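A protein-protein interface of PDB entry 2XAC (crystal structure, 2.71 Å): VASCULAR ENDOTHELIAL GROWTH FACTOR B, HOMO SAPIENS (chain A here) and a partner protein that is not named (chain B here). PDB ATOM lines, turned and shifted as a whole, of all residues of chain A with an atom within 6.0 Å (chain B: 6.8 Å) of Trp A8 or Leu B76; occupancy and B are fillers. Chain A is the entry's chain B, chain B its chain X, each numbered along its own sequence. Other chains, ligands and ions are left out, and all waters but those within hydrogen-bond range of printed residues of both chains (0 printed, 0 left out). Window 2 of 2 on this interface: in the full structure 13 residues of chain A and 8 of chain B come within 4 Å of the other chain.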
ATOM      1  N   VAL A   6      11.619 -36.343  36.896  1.00  0.00           N
ATOM      2  CA  VAL A   6      12.716 -35.872  36.045  1.00  0.00           C
ATOM      3  C   VAL A   6      12.173 -34.791  35.128  1.00  0.00           C
ATOM      4  O   VAL A   6      11.248 -35.035  34.356  1.00  0.00           O
ATOM      5  CB  VAL A   6      13.360 -37.005  35.222  1.00  0.00           C
ATOM      6  CG1 VAL A   6      14.393 -36.442  34.256  1.00  0.00           C
ATOM      7  CG2 VAL A   6      14.007 -38.035  36.144  1.00  0.00           C
ATOM      8  N   SER A   7      12.739 -33.593  35.246  1.00  0.00           N
ATOM      9  CA  SER A   7      12.226 -32.418  34.554  1.00  0.00           C
ATOM     10  C   SER A   7      12.342 -32.578  33.054  1.00  0.00           C
ATOM     11  O   SER A   7      13.288 -33.202  32.574  1.00  0.00           O
ATOM     12  CB  SER A   7      12.986 -31.183  34.998  1.00  0.00           C
ATOM     13  OG  SER A   7      12.229 -30.024  34.710  1.00  0.00           O
ATOM     14  N   TRP A   8      11.395 -32.009  32.314  1.00  0.00           N
ATOM     15  CA  TRP A   8      11.349 -32.207  30.869  1.00  0.00           C
ATOM     16  C   TRP A   8      12.678 -31.930  30.179  1.00  0.00           C
ATOM     17  O   TRP A   8      13.153 -32.755  29.397  1.00  0.00           O
ATOM     18  CB  TRP A   8      10.255 -31.386  30.201  1.00  0.00           C
ATOM     19  CG  TRP A   8      10.226 -31.654  28.722  1.00  0.00           C
ATOM     20  CD1 TRP A   8       9.672 -32.737  28.097  1.00  0.00           C
ATOM     21  CD2 TRP A   8      10.813 -30.853  27.690  1.00  0.00           C
ATOM     22  NE1 TRP A   8       9.866 -32.651  26.740  1.00  0.00           N
ATOM     23  CE2 TRP A   8      10.562 -31.504  26.462  1.00  0.00           C
ATOM     24  CE3 TRP A   8      11.520 -29.641  27.683  1.00  0.00           C
ATOM     25  CZ2 TRP A   8      10.990 -30.985  25.234  1.00  0.00           C
ATOM     26  CZ3 TRP A   8      11.946 -29.123  26.458  1.00  0.00           C
ATOM     27  CH2 TRP A   8      11.679 -29.799  25.253  1.00  0.00           C
ATOM     28  N   ILE A   9      13.257 -30.765  30.466  1.00  0.00           N
ATOM     29  CA  ILE A   9      14.587 -30.398  29.986  1.00  0.00           C
ATOM     30  C   ILE A   9      15.547 -31.577  30.000  1.00  0.00           C
ATOM     31  O   ILE A   9      16.238 -31.824  29.017  1.00  0.00           O
ATOM     32  CB  ILE A   9      15.203 -29.236  30.810  1.00  0.00           C
ATOM     33  CG1 ILE A   9      14.765 -29.320  32.279  1.00  0.00           C
ATOM     34  CG2 ILE A   9      14.812 -27.890  30.206  1.00  0.00           C
ATOM     35  CD1 ILE A   9      15.613 -28.498  33.235  1.00  0.00           C
ATOM     36  N   ASP A  10      15.573 -32.312  31.109  1.00  0.00           N
ATOM     37  CA  ASP A  10      16.510 -33.418  31.276  1.00  0.00           C
ATOM     38  C   ASP A  10      16.033 -34.662  30.561  1.00  0.00           C
ATOM     39  O   ASP A  10      16.843 -35.437  30.052  1.00  0.00           O
ATOM     40  CB  ASP A  10      16.734 -33.716  32.752  1.00  0.00           C
ATOM     41  CG  ASP A  10      17.191 -32.506  33.518  1.00  0.00           C
ATOM     42  OD1 ASP A  10      16.696 -32.316  34.646  1.00  0.00           O
ATOM     43  OD2 ASP A  10      18.027 -31.736  32.992  1.00  0.00           O
ATOM     44  N   VAL A  11      14.716 -34.855  30.533  1.00  0.00           N
ATOM     45  CA  VAL A  11      14.138 -35.954  29.778  1.00  0.00           C
ATOM     46  C   VAL A  11      14.574 -35.774  28.330  1.00  0.00           C
ATOM     47  O   VAL A  11      15.066 -36.716  27.706  1.00  0.00           O
ATOM     48  CB  VAL A  11      12.599 -35.999  29.870  1.00  0.00           C
ATOM     49  CG1 VAL A  11      12.065 -37.264  29.206  1.00  0.00           C
ATOM     50  CG2 VAL A  11      12.143 -35.941  31.313  1.00  0.00           C
ATOM     51  N   TYR A  12      14.425 -34.555  27.816  1.00  0.00           N
ATOM     52  CA  TYR A  12      14.844 -34.250  26.455  1.00  0.00           C
ATOM     53  C   TYR A  12      16.361 -34.334  26.307  1.00  0.00           C
ATOM     54  O   TYR A  12      16.860 -35.002  25.403  1.00  0.00           O
ATOM     55  CB  TYR A  12      14.336 -32.880  26.009  1.00  0.00           C
ATOM     56  CG  TYR A  12      14.932 -32.439  24.694  1.00  0.00           C
ATOM     57  CD1 TYR A  12      14.262 -32.680  23.493  1.00  0.00           C
ATOM     58  CD2 TYR A  12      16.168 -31.794  24.646  1.00  0.00           C
ATOM     59  CE1 TYR A  12      14.804 -32.289  22.278  1.00  0.00           C
ATOM     60  CE2 TYR A  12      16.720 -31.398  23.436  1.00  0.00           C
ATOM     61  CZ  TYR A  12      16.029 -31.650  22.256  1.00  0.00           C
ATOM     62  OH  TYR A  12      16.559 -31.266  21.045  1.00  0.00           O
ATOM     63  N   THR A  13      17.083 -33.661  27.197  1.00  0.00           N
ATOM     64  CA  THR A  13      18.539 -33.711  27.211  1.00  0.00           C
ATOM     65  C   THR A  13      18.987 -35.164  27.108  1.00  0.00           C
ATOM     66  O   THR A  13      19.667 -35.543  26.160  1.00  0.00           O
ATOM     67  CB  THR A  13      19.105 -33.014  28.482  1.00  0.00           C
ATOM     68  OG1 THR A  13      18.862 -31.605  28.389  1.00  0.00           O
ATOM     69  CG2 THR A  13      20.604 -33.251  28.649  1.00  0.00           C
ATOM     70  N   PRO A  53      14.244 -35.430  16.055  1.00  0.00           N
ATOM     71  CA  PRO A  53      12.987 -34.677  16.018  1.00  0.00           C
ATOM     72  C   PRO A  53      11.808 -35.343  15.302  1.00  0.00           C
ATOM     73  O   PRO A  53      10.664 -35.153  15.724  1.00  0.00           O
ATOM     74  CB  PRO A  53      13.382 -33.398  15.289  1.00  0.00           C
ATOM     75  CG  PRO A  53      14.773 -33.183  15.682  1.00  0.00           C
ATOM     76  CD  PRO A  53      15.400 -34.531  15.858  1.00  0.00           C
ATOM     77  N   TYR B  11      10.572 -16.904  31.836  1.00  0.00           N
ATOM     78  CA  TYR B  11      10.910 -18.298  31.574  1.00  0.00           C
ATOM     79  C   TYR B  11       9.694 -19.207  31.654  1.00  0.00           C
ATOM     80  O   TYR B  11       8.870 -19.097  32.569  1.00  0.00           O
ATOM     81  CB  TYR B  11      12.011 -18.829  32.498  1.00  0.00           C
ATOM     82  CG  TYR B  11      12.381 -20.258  32.161  1.00  0.00           C
ATOM     83  CD1 TYR B  11      13.189 -20.546  31.058  1.00  0.00           C
ATOM     84  CD2 TYR B  11      11.891 -21.325  32.916  1.00  0.00           C
ATOM     85  CE1 TYR B  11      13.520 -21.857  30.727  1.00  0.00           C
ATOM     86  CE2 TYR B  11      12.215 -22.645  32.593  1.00  0.00           C
ATOM     87  CZ  TYR B  11      13.031 -22.901  31.498  1.00  0.00           C
ATOM     88  OH  TYR B  11      13.355 -24.198  31.169  1.00  0.00           O
ATOM     89  N   GLU B  13       8.694 -23.488  31.318  1.00  0.00           N
ATOM     90  CA  GLU B  13       9.098 -24.881  31.163  1.00  0.00           C
ATOM     91  C   GLU B  13       8.725 -25.337  29.753  1.00  0.00           C
ATOM     92  O   GLU B  13       9.450 -26.112  29.125  1.00  0.00           O
ATOM     93  CB  GLU B  13       8.414 -25.769  32.205  1.00  0.00           C
ATOM     94  CG  GLU B  13       8.872 -25.543  33.643  1.00  0.00           C
ATOM     95  CD  GLU B  13       8.632 -26.754  34.537  1.00  0.00           C
ATOM     96  OE1 GLU B  13       9.390 -27.748  34.430  1.00  0.00           O
ATOM     97  OE2 GLU B  13       7.689 -26.705  35.355  1.00  0.00           O
ATOM     98  N   ILE B  14       7.590 -24.837  29.269  1.00  0.00           N
ATOM     99  CA  ILE B  14       7.157 -25.042  27.895  1.00  0.00           C
ATOM    100  C   ILE B  14       7.934 -24.099  26.970  1.00  0.00           C
ATOM    101  O   ILE B  14       7.885 -22.877  27.143  1.00  0.00           O
ATOM    102  CB  ILE B  14       5.637 -24.774  27.724  1.00  0.00           C
ATOM    103  CG1 ILE B  14       4.824 -25.380  28.882  1.00  0.00           C
ATOM    104  CG2 ILE B  14       5.150 -25.230  26.342  1.00  0.00           C
ATOM    105  CD1 ILE B  14       4.976 -26.882  29.077  1.00  0.00           C
ATOM    106  N   PRO B  15       8.661 -24.664  25.989  1.00  0.00           N
ATOM    107  CA  PRO B  15       9.338 -23.829  25.004  1.00  0.00           C
ATOM    108  C   PRO B  15       8.355 -23.320  23.948  1.00  0.00           C
ATOM    109  O   PRO B  15       7.301 -23.933  23.739  1.00  0.00           O
ATOM    110  CB  PRO B  15      10.352 -24.789  24.380  1.00  0.00           C
ATOM    111  CG  PRO B  15       9.725 -26.121  24.494  1.00  0.00           C
ATOM    112  CD  PRO B  15       8.905 -26.101  25.756  1.00  0.00           C
ATOM    113  N   LYS B  42      22.333 -21.654  21.409  1.00  0.00           N
ATOM    114  CA  LYS B  42      22.882 -22.991  21.595  1.00  0.00           C
ATOM    115  C   LYS B  42      21.923 -24.050  21.060  1.00  0.00           C
ATOM    116  O   LYS B  42      20.730 -23.793  20.871  1.00  0.00           O
ATOM    117  CB  LYS B  42      23.181 -23.251  23.072  1.00  0.00           C
ATOM    118  CG  LYS B  42      24.065 -24.465  23.311  1.00  0.00           C
ATOM    119  CD  LYS B  42      23.514 -25.321  24.434  1.00  0.00           C
ATOM    120  CE  LYS B  42      24.149 -26.698  24.427  1.00  0.00           C
ATOM    121  NZ  LYS B  42      23.543 -27.555  25.482  1.00  0.00           N
ATOM    122  N   LYS B  43      22.455 -25.242  20.826  1.00  0.00           N
ATOM    123  CA  LYS B  43      21.672 -26.346  20.313  1.00  0.00           C
ATOM    124  C   LYS B  43      22.249 -27.646  20.853  1.00  0.00           C
ATOM    125  O   LYS B  43      23.233 -28.163  20.315  1.00  0.00           O
ATOM    126  CB  LYS B  43      21.703 -26.321  18.784  1.00  0.00           C
ATOM    127  CG  LYS B  43      20.691 -27.228  18.090  1.00  0.00           C
ATOM    128  CD  LYS B  43      20.449 -26.782  16.640  1.00  0.00           C
ATOM    129  CE  LYS B  43      21.738 -26.718  15.806  1.00  0.00           C
ATOM    130  NZ  LYS B  43      21.521 -26.100  14.462  1.00  0.00           N
ATOM    131  N   PHE B  44      21.653 -28.151  21.933  1.00  0.00           N
ATOM    132  CA  PHE B  44      22.045 -29.435  22.516  1.00  0.00           C
ATOM    133  C   PHE B  44      21.910 -30.553  21.470  1.00  0.00           C
ATOM    134  O   PHE B  44      20.910 -30.593  20.744  1.00  0.00           O
ATOM    135  CB  PHE B  44      21.205 -29.756  23.762  1.00  0.00           C
ATOM    136  CG  PHE B  44      21.706 -30.948  24.538  1.00  0.00           C
ATOM    137  CD1 PHE B  44      22.666 -30.789  25.539  1.00  0.00           C
ATOM    138  CD2 PHE B  44      21.232 -32.232  24.257  1.00  0.00           C
ATOM    139  CE1 PHE B  44      23.148 -31.894  26.257  1.00  0.00           C
ATOM    140  CE2 PHE B  44      21.708 -33.337  24.966  1.00  0.00           C
ATOM    141  CZ  PHE B  44      22.668 -33.169  25.969  1.00  0.00           C
ATOM    142  N   GLU B  73      18.913 -27.237  11.972  1.00  0.00           N
ATOM    143  CA  GLU B  73      18.083 -26.357  12.785  1.00  0.00           C
ATOM    144  C   GLU B  73      16.784 -26.981  13.295  1.00  0.00           C
ATOM    145  O   GLU B  73      16.037 -26.319  14.011  1.00  0.00           O
ATOM    146  CB  GLU B  73      17.774 -25.063  12.027  1.00  0.00           C
ATOM    147  CG  GLU B  73      18.920 -24.069  11.997  1.00  0.00           C
ATOM    148  CD  GLU B  73      19.957 -24.412  10.957  1.00  0.00           C
ATOM    149  OE1 GLU B  73      19.707 -24.130   9.770  1.00  0.00           O
ATOM    150  OE2 GLU B  73      21.021 -24.955  11.329  1.00  0.00           O
ATOM    151  N   ILE B  74      16.507 -28.233  12.923  1.00  0.00           N
ATOM    152  CA  ILE B  74      15.322 -28.935  13.435  1.00  0.00           C
ATOM    153  C   ILE B  74      15.652 -29.556  14.786  1.00  0.00           C
ATOM    154  O   ILE B  74      16.621 -30.318  14.916  1.00  0.00           O
ATOM    155  CB  ILE B  74      14.783 -30.042  12.479  1.00  0.00           C
ATOM    156  CG1 ILE B  74      14.723 -29.560  11.029  1.00  0.00           C
ATOM    157  CG2 ILE B  74      13.394 -30.529  12.940  1.00  0.00           C
ATOM    158  CD1 ILE B  74      14.683 -30.683  10.027  1.00  0.00           C
ATOM    159  N   GLY B  75      14.833 -29.231  15.780  1.00  0.00           N
ATOM    160  CA  GLY B  75      15.061 -29.649  17.161  1.00  0.00           C
ATOM    161  C   GLY B  75      14.984 -28.467  18.110  1.00  0.00           C
ATOM    162  O   GLY B  75      14.334 -27.462  17.814  1.00  0.00           O
ATOM    163  N   LEU B  76      15.648 -28.585  19.254  1.00  0.00           N
ATOM    164  CA  LEU B  76      15.577 -27.554  20.292  1.00  0.00           C
ATOM    165  C   LEU B  76      16.693 -26.527  20.160  1.00  0.00           C
ATOM    166  O   LEU B  76      17.876 -26.878  20.100  1.00  0.00           O
ATOM    167  CB  LEU B  76      15.572 -28.195  21.690  1.00  0.00           C
ATOM    168  CG  LEU B  76      15.809 -27.337  22.934  1.00  0.00           C
ATOM    169  CD1 LEU B  76      14.812 -27.664  24.025  1.00  0.00           C
ATOM    170  CD2 LEU B  76      17.246 -27.508  23.428  1.00  0.00           C
ATOM    171  N   LEU B  77      16.305 -25.258  20.113  1.00  0.00           N
ATOM    172  CA  LEU B  77      17.274 -24.165  20.059  1.00  0.00           C
ATOM    173  C   LEU B  77      17.138 -23.289  21.297  1.00  0.00           C
ATOM    174  O   LEU B  77      16.041 -22.870  21.662  1.00  0.00           O
ATOM    175  CB  LEU B  77      17.119 -23.342  18.772  1.00  0.00           C
ATOM    176  CG  LEU B  77      17.447 -24.044  17.449  1.00  0.00           C
ATOM    177  CD1 LEU B  77      16.253 -24.817  16.941  1.00  0.00           C
ATOM    178  CD2 LEU B  77      17.877 -23.037  16.400  1.00  0.00           C
ATOM    179  N   THR B  78      18.257 -23.030  21.954  1.00  0.00           N
ATOM    180  CA  THR B  78      18.212 -22.317  23.223  1.00  0.00           C
ATOM    181  C   THR B  78      19.021 -21.030  23.168  1.00  0.00           C
ATOM    182  O   THR B  78      20.243 -21.059  23.026  1.00  0.00           O
ATOM    183  CB  THR B  78      18.700 -23.214  24.396  1.00  0.00           C
ATOM    184  OG1 THR B  78      18.073 -24.503  24.322  1.00  0.00           O
ATOM    185  CG2 THR B  78      18.361 -22.582  25.725  1.00  0.00           C
ATOM    186  N   ASN B  91      14.342 -21.674  25.798  1.00  0.00           N
ATOM    187  CA  ASN B  91      14.276 -22.823  24.909  1.00  0.00           C
ATOM    188  C   ASN B  91      13.245 -22.644  23.795  1.00  0.00           C
ATOM    189  O   ASN B  91      12.163 -22.099  24.020  1.00  0.00           O
ATOM    190  CB  ASN B  91      14.010 -24.097  25.721  1.00  0.00           C
ATOM    191  CG  ASN B  91      13.415 -23.811  27.109  1.00  0.00           C
ATOM    192  OD1 ASN B  91      13.960 -24.248  28.128  1.00  0.00           O
ATOM    193  ND2 ASN B  91      12.298 -23.073  27.152  1.00  0.00           N
ATOM    194  N   TYR B  92      13.607 -23.087  22.593  1.00  0.00           N
ATOM    195  CA  TYR B  92      12.740 -22.997  21.419  1.00  0.00           C
ATOM    196  C   TYR B  92      12.731 -24.319  20.657  1.00  0.00           C
ATOM    197  O   TYR B  92      13.779 -24.799  20.216  1.00  0.00           O
ATOM    198  CB  TYR B  92      13.222 -21.884  20.482  1.00  0.00           C
ATOM    199  CG  TYR B  92      13.011 -20.488  21.003  1.00  0.00           C
ATOM    200  CD1 TYR B  92      13.994 -19.844  21.753  1.00  0.00           C
ATOM    201  CD2 TYR B  92      11.829 -19.805  20.739  1.00  0.00           C
ATOM    202  CE1 TYR B  92      13.794 -18.553  22.235  1.00  0.00           C
ATOM    203  CE2 TYR B  92      11.618 -18.525  21.216  1.00  0.00           C
ATOM    204  CZ  TYR B  92      12.604 -17.902  21.957  1.00  0.00           C
ATOM    205  OH  TYR B  92      12.382 -16.632  22.424  1.00  0.00           O
ATOM    206  N   LEU B  93      11.550 -24.905  20.501  1.00  0.00           N
ATOM    207  CA  LEU B  93      11.421 -26.167  19.778  1.00  0.00           C
ATOM    208  C   LEU B  93      10.990 -25.907  18.345  1.00  0.00           C
ATOM    209  O   LEU B  93       9.940 -25.303  18.101  1.00  0.00           O
ATOM    210  CB  LEU B  93      10.402 -27.077  20.470  1.00  0.00           C
ATOM    211  CG  LEU B  93      10.552 -28.603  20.412  1.00  0.00           C
ATOM    212  CD1 LEU B  93       9.635 -29.208  21.447  1.00  0.00           C
ATOM    213  CD2 LEU B  93      10.257 -29.206  19.037  1.00  0.00           C
ATOM    214  N   THR B  94      11.798 -26.360  17.397  1.00  0.00           N
ATOM    215  CA  THR B  94      11.410 -26.269  15.994  1.00  0.00           C
ATOM    216  C   THR B  94      11.001 -27.630  15.434  1.00  0.00           C
ATOM    217  O   THR B  94      11.578 -28.664  15.784  1.00  0.00           O
ATOM    218  CB  THR B  94      12.516 -25.649  15.117  1.00  0.00           C
ATOM    219  OG1 THR B  94      13.616 -26.557  15.010  1.00  0.00           O
ATOM    220  CG2 THR B  94      12.994 -24.326  15.699  1.00  0.00           C
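OH of Tyr A12 sits close to N of Leu B76, 3.4 Å away.
OG1 of Thr A13 lies within hydrogen-bond range of O of Ile A9 (2.7 Å). The backbone carbonyl oxygen of Gly B75 lies within hydrogen-bond range of the backbone NH of Thr B94, at 2.8 Å.
Among the printed residues, pairs that only touch across the chains: Ser A7 with Glu B13 (3.6 Å), Trp A8 with Leu B76 (3.99 Å), Thr A13 with Phe B44 (3.2 Å), Pro A53 with Ile B74 (3.5 Å) and Pro A53 with Gly B75 (3.8 Å).
Printed residues of chain A within 4 Å of Leu B76: Trp A8 and Tyr A12. Of the printed residues of chain A, Gly B75 touches Pro A53 (3.8 Å). Printed residues of chain B within 4 Å of Ser A7: Glu B13. Printed residues of chain A within 4 Å of Ile B74: Pro A53 (3.5 Å). Printed residues of chain B within 4 Å of Tyr A12: Leu B76 (3.3 Å). Of the printed residues of chain A, Glu B13 touches Ser A7. Thr B94 touches none of the printed residues of chain A. The nearest printed residue of chain B that does not touch Trp A8 is Pro B15 (4.2 Å). The nearest printed residue of chain A that does not touch Leu B76 is Pro A53 (5.9 Å).
Printed residues of chain B that touch a printed residue of chain A: Glu B13, Phe B44, Ile B74, Gly B75 and Leu B76. Hydrophobic or aromatic side chains of chain B within 4 Å of the printed part of chain A: Phe B44, Ile B74 and Leu B76. Among the printed residues, no Asp or Glu carboxylate lies within 4 Å of a Lys or Arg side-chain nitrogen of the other chain.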
